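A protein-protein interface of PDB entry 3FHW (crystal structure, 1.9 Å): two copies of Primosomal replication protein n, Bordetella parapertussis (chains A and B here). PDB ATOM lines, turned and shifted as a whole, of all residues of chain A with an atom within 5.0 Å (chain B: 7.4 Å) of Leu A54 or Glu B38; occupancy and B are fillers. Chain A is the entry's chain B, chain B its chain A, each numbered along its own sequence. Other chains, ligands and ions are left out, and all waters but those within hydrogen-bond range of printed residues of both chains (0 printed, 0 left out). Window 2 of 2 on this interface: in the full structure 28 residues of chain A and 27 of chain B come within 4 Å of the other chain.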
ATOM      1  N   THR A  19     -19.394 -20.367  -6.464  1.00  0.00           N
ATOM      2  CA  THR A  19     -20.071 -21.393  -5.670  1.00  0.00           C
ATOM      3  C   THR A  19     -21.406 -20.833  -5.185  1.00  0.00           C
ATOM      4  O   THR A  19     -21.592 -19.604  -5.152  1.00  0.00           O
ATOM      5  CB  THR A  19     -19.225 -21.849  -4.458  1.00  0.00           C
ATOM      6  OG1 THR A  19     -19.108 -20.774  -3.520  1.00  0.00           O
ATOM      7  CG2 THR A  19     -17.833 -22.304  -4.900  1.00  0.00           C
ATOM      8  N   LEU A  23     -18.241 -17.884  -3.530  1.00  0.00           N
ATOM      9  CA  LEU A  23     -16.799 -17.963  -3.742  1.00  0.00           C
ATOM     10  C   LEU A  23     -16.457 -18.093  -5.227  1.00  0.00           C
ATOM     11  O   LEU A  23     -17.151 -18.812  -5.959  1.00  0.00           O
ATOM     12  CB  LEU A  23     -16.213 -19.154  -2.974  1.00  0.00           C
ATOM     13  CG  LEU A  23     -14.738 -19.095  -2.564  1.00  0.00           C
ATOM     14  CD1 LEU A  23     -14.499 -17.976  -1.530  1.00  0.00           C
ATOM     15  CD2 LEU A  23     -14.298 -20.441  -2.016  1.00  0.00           C
ATOM     16  N   PRO A  24     -15.388 -17.398  -5.688  1.00  0.00           N
ATOM     17  CA  PRO A  24     -14.908 -17.608  -7.051  1.00  0.00           C
ATOM     18  C   PRO A  24     -14.725 -19.092  -7.375  1.00  0.00           C
ATOM     19  O   PRO A  24     -14.250 -19.849  -6.532  1.00  0.00           O
ATOM     20  CB  PRO A  24     -13.545 -16.896  -7.055  1.00  0.00           C
ATOM     21  CG  PRO A  24     -13.687 -15.820  -6.037  1.00  0.00           C
ATOM     22  CD  PRO A  24     -14.607 -16.367  -4.976  1.00  0.00           C
ATOM     23  N   ALA A  25     -15.140 -19.493  -8.574  1.00  0.00           N
ATOM     24  CA  ALA A  25     -14.982 -20.858  -9.072  1.00  0.00           C
ATOM     25  C   ALA A  25     -14.672 -20.823 -10.565  1.00  0.00           C
ATOM     26  O   ALA A  25     -15.234 -20.009 -11.310  1.00  0.00           O
ATOM     27  CB  ALA A  25     -16.265 -21.680  -8.815  1.00  0.00           C
ATOM     28  N   VAL A  52     -11.496 -28.136 -11.286  1.00  0.00           N
ATOM     29  CA  VAL A  52     -12.136 -26.937 -10.738  1.00  0.00           C
ATOM     30  C   VAL A  52     -11.250 -26.347  -9.643  1.00  0.00           C
ATOM     31  O   VAL A  52     -10.738 -27.069  -8.782  1.00  0.00           O
ATOM     32  CB  VAL A  52     -13.606 -27.212 -10.232  1.00  0.00           C
ATOM     33  CG1 VAL A  52     -13.650 -28.340  -9.209  1.00  0.00           C
ATOM     34  CG2 VAL A  52     -14.251 -25.955  -9.643  1.00  0.00           C
ATOM     35  N   ALA A  53     -11.075 -25.029  -9.706  1.00  0.00           N
ATOM     36  CA  ALA A  53     -10.338 -24.288  -8.709  1.00  0.00           C
ATOM     37  C   ALA A  53     -11.335 -23.362  -8.024  1.00  0.00           C
ATOM     38  O   ALA A  53     -12.229 -22.814  -8.682  1.00  0.00           O
ATOM     39  CB  ALA A  53      -9.226 -23.476  -9.368  1.00  0.00           C
ATOM     40  N   LEU A  54     -11.192 -23.218  -6.710  1.00  0.00           N
ATOM     41  CA  LEU A  54     -12.051 -22.324  -5.932  1.00  0.00           C
ATOM     42  C   LEU A  54     -11.207 -21.279  -5.233  1.00  0.00           C
ATOM     43  O   LEU A  54     -10.032 -21.511  -4.942  1.00  0.00           O
ATOM     44  CB  LEU A  54     -12.892 -23.100  -4.899  1.00  0.00           C
ATOM     45  CG  LEU A  54     -13.902 -24.161  -5.331  1.00  0.00           C
ATOM     46  CD1 LEU A  54     -14.772 -24.551  -4.140  1.00  0.00           C
ATOM     47  CD2 LEU A  54     -14.762 -23.703  -6.479  1.00  0.00           C
ATOM     48  N   GLY A  55     -11.810 -20.124  -4.973  1.00  0.00           N
ATOM     49  CA  GLY A  55     -11.161 -19.076  -4.216  1.00  0.00           C
ATOM     50  C   GLY A  55     -10.056 -18.386  -4.976  1.00  0.00           C
ATOM     51  O   GLY A  55     -10.199 -18.059  -6.167  1.00  0.00           O
ATOM     52  N   ASP A  56      -8.944 -18.185  -4.280  1.00  0.00           N
ATOM     53  CA  ASP A  56      -7.808 -17.440  -4.811  1.00  0.00           C
ATOM     54  C   ASP A  56      -7.135 -18.124  -6.003  1.00  0.00           C
ATOM     55  O   ASP A  56      -6.678 -17.440  -6.917  1.00  0.00           O
ATOM     56  CB  ASP A  56      -6.794 -17.157  -3.697  1.00  0.00           C
ATOM     57  CG  ASP A  56      -7.271 -16.081  -2.724  1.00  0.00           C
ATOM     58  OD1 ASP A  56      -8.376 -15.522  -2.923  1.00  0.00           O
ATOM     59  OD2 ASP A  56      -6.539 -15.801  -1.749  1.00  0.00           O
ATOM     60  N   LEU A  57      -7.091 -19.461  -6.001  1.00  0.00           N
ATOM     61  CA  LEU A  57      -6.552 -20.214  -7.148  1.00  0.00           C
ATOM     62  C   LEU A  57      -7.409 -20.031  -8.399  1.00  0.00           C
ATOM     63  O   LEU A  57      -6.887 -19.952  -9.510  1.00  0.00           O
ATOM     64  CB  LEU A  57      -6.402 -21.697  -6.824  1.00  0.00           C
ATOM     65  CG  LEU A  57      -5.541 -22.534  -7.777  1.00  0.00           C
ATOM     66  CD1 LEU A  57      -4.165 -21.896  -8.039  1.00  0.00           C
ATOM     67  CD2 LEU A  57      -5.385 -23.913  -7.177  1.00  0.00           C
ATOM     68  N   ALA A  58      -8.720 -19.941  -8.218  1.00  0.00           N
ATOM     69  CA  ALA A  58      -9.617 -19.628  -9.320  1.00  0.00           C
ATOM     70  C   ALA A  58      -9.273 -18.255  -9.913  1.00  0.00           C
ATOM     71  O   ALA A  58      -9.178 -18.102 -11.135  1.00  0.00           O
ATOM     72  CB  ALA A  58     -11.078 -19.677  -8.862  1.00  0.00           C
ATOM     73  N   PHE A  75      -7.350 -32.937  -5.084  1.00  0.00           N
ATOM     74  CA  PHE A  75      -8.080 -34.158  -4.744  1.00  0.00           C
ATOM     75  C   PHE A  75      -9.127 -34.514  -5.789  1.00  0.00           C
ATOM     76  O   PHE A  75      -9.688 -33.643  -6.447  1.00  0.00           O
ATOM     77  CB  PHE A  75      -8.686 -34.094  -3.330  1.00  0.00           C
ATOM     78  CG  PHE A  75      -9.760 -33.051  -3.150  1.00  0.00           C
ATOM     79  CD1 PHE A  75     -11.098 -33.357  -3.422  1.00  0.00           C
ATOM     80  CD2 PHE A  75      -9.443 -31.783  -2.684  1.00  0.00           C
ATOM     81  CE1 PHE A  75     -12.099 -32.409  -3.243  1.00  0.00           C
ATOM     82  CE2 PHE A  75     -10.442 -30.813  -2.498  1.00  0.00           C
ATOM     83  CZ  PHE A  75     -11.770 -31.130  -2.781  1.00  0.00           C
ATOM     84  N   HIS A  89     -10.205 -31.468  -8.000  1.00  0.00           N
ATOM     85  CA  HIS A  89     -10.359 -30.238  -7.247  1.00  0.00           C
ATOM     86  C   HIS A  89      -8.977 -29.693  -6.962  1.00  0.00           C
ATOM     87  O   HIS A  89      -8.263 -30.195  -6.104  1.00  0.00           O
ATOM     88  CB  HIS A  89     -11.180 -30.477  -5.985  1.00  0.00           C
ATOM     89  CG  HIS A  89     -12.640 -30.649  -6.256  1.00  0.00           C
ATOM     90  ND1 HIS A  89     -13.137 -31.716  -6.966  1.00  0.00           N
ATOM     91  CD2 HIS A  89     -13.704 -29.874  -5.944  1.00  0.00           C
ATOM     92  CE1 HIS A  89     -14.449 -31.591  -7.084  1.00  0.00           C
ATOM     93  NE2 HIS A  89     -14.817 -30.484  -6.467  1.00  0.00           N
ATOM     94  N   VAL B  36     -11.189 -33.187   3.249  1.00  0.00           N
ATOM     95  CA  VAL B  36     -10.033 -32.505   2.676  1.00  0.00           C
ATOM     96  C   VAL B  36     -10.200 -31.006   2.889  1.00  0.00           C
ATOM     97  O   VAL B  36     -11.227 -30.567   3.410  1.00  0.00           O
ATOM     98  CB  VAL B  36      -9.893 -32.810   1.170  1.00  0.00           C
ATOM     99  CG1 VAL B  36      -9.418 -34.243   0.955  1.00  0.00           C
ATOM    100  CG2 VAL B  36     -11.225 -32.584   0.461  1.00  0.00           C
ATOM    101  N   VAL B  37      -9.188 -30.232   2.503  1.00  0.00           N
ATOM    102  CA  VAL B  37      -9.264 -28.774   2.579  1.00  0.00           C
ATOM    103  C   VAL B  37      -9.312 -28.177   1.173  1.00  0.00           C
ATOM    104  O   VAL B  37      -8.486 -28.499   0.314  1.00  0.00           O
ATOM    105  CB  VAL B  37      -8.135 -28.159   3.485  1.00  0.00           C
ATOM    106  CG1 VAL B  37      -6.778 -28.816   3.221  1.00  0.00           C
ATOM    107  CG2 VAL B  37      -8.061 -26.633   3.338  1.00  0.00           C
ATOM    108  N   GLU B  38     -10.332 -27.359   0.933  1.00  0.00           N
ATOM    109  CA  GLU B  38     -10.501 -26.667  -0.342  1.00  0.00           C
ATOM    110  C   GLU B  38     -10.817 -25.184  -0.109  1.00  0.00           C
ATOM    111  O   GLU B  38     -11.802 -24.855   0.560  1.00  0.00           O
ATOM    112  CB  GLU B  38     -11.605 -27.333  -1.170  1.00  0.00           C
ATOM    113  CG  GLU B  38     -11.656 -26.849  -2.615  1.00  0.00           C
ATOM    114  CD  GLU B  38     -12.777 -27.473  -3.427  1.00  0.00           C
ATOM    115  OE1 GLU B  38     -13.811 -27.874  -2.844  1.00  0.00           O
ATOM    116  OE2 GLU B  38     -12.628 -27.528  -4.665  1.00  0.00           O
ATOM    117  N   ALA B  39      -9.982 -24.306  -0.675  1.00  0.00           N
ATOM    118  CA  ALA B  39     -10.091 -22.842  -0.512  1.00  0.00           C
ATOM    119  C   ALA B  39     -10.287 -22.399   0.937  1.00  0.00           C
ATOM    120  O   ALA B  39     -11.274 -21.732   1.275  1.00  0.00           O
ATOM    121  CB  ALA B  39     -11.186 -22.263  -1.410  1.00  0.00           C
ATOM    122  N   GLY B  40      -9.331 -22.775   1.786  1.00  0.00           N
ATOM    123  CA  GLY B  40      -9.300 -22.330   3.172  1.00  0.00           C
ATOM    124  C   GLY B  40      -9.912 -23.329   4.135  1.00  0.00           C
ATOM    125  O   GLY B  40     -10.180 -22.998   5.292  1.00  0.00           O
ATOM    126  N   ARG B  43     -14.502 -29.638   3.710  1.00  0.00           N
ATOM    127  CA  ARG B  43     -15.243 -30.391   2.708  1.00  0.00           C
ATOM    128  C   ARG B  43     -15.006 -31.879   2.910  1.00  0.00           C
ATOM    129  O   ARG B  43     -13.875 -32.312   3.145  1.00  0.00           O
ATOM    130  CB  ARG B  43     -14.794 -29.999   1.296  1.00  0.00           C
ATOM    131  CG  ARG B  43     -15.735 -30.459   0.173  1.00  0.00           C
ATOM    132  CD  ARG B  43     -14.958 -31.069  -0.979  1.00  0.00           C
ATOM    133  NE  ARG B  43     -15.647 -30.946  -2.266  1.00  0.00           N
ATOM    134  CZ  ARG B  43     -16.392 -31.897  -2.827  1.00  0.00           C
ATOM    135  NH1 ARG B  43     -16.970 -31.674  -4.006  1.00  0.00           N
ATOM    136  NH2 ARG B  43     -16.566 -33.071  -2.223  1.00  0.00           N
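The guanidinium group of Arg B43 is in hydrogen-bond range of a ring nitrogen (NE2) of His A89.
Leu A54 touches just these residues of chain B: Glu B38 (3.6 Å) and Ala B39 (3.8 Å).
Of the printed residues of chain B, Phe A75 touches Val B36 (3.5 Å), Glu B38 (3.8 Å) and Arg B43 (3.7 Å).
Printed residues of chain B within 4 Å of His A89: Glu B38 (2.9 Å) and Arg B43 (3.5 Å).
Of the printed residues of chain A, Ala B39 touches Leu A23 (3.7 Å) and Leu A54 (3.8 Å).
Printed residues of chain A within 4 Å of Arg B43: Phe A75 (3.7 Å) and His A89 (3.5 Å).
The nearest residue of chain B that does not touch Leu A54 is Arg B43 (6.7 Å).
The nearest residue of chain A that does not touch Glu B38 is Val A52 (4.6 Å).
Among the printed residues, pairs that only touch across the chains: His A89 with Glu B38, Phe A75 with Val B36, Leu A54 with Glu B38, Leu A23 with Ala B39, Phe A75 with Arg B43, Leu A54 with Ala B39 and Phe A75 with Glu B38.
No position is printed for both chains.
Of the 8 pairs that touch across the chains among the printed residues, none has its exchanged pair printed and touching as well.
Of the 13 printed residues of chain A, 4 touch a printed residue of chain B.
Among the printed residues, 8 pairs touch across the chains.
Among the printed residues, no Asp or Glu carboxylate lies within 4 Å of a Lys or Arg side-chain nitrogen of the other chain.
N of Val B36 lies within hydrogen-bond range of O of Arg B43 (2.8 Å).
NE of Arg B43 lies within salt-bridge range of OE1 of Glu B38 (3.6 Å).
N of Leu A23 sits at hydrogen-bond distance from OG1 of Thr A19 (3.0 Å).
O of Phe A75 sits at hydrogen-bond distance from N of His A89 (2.7 Å).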
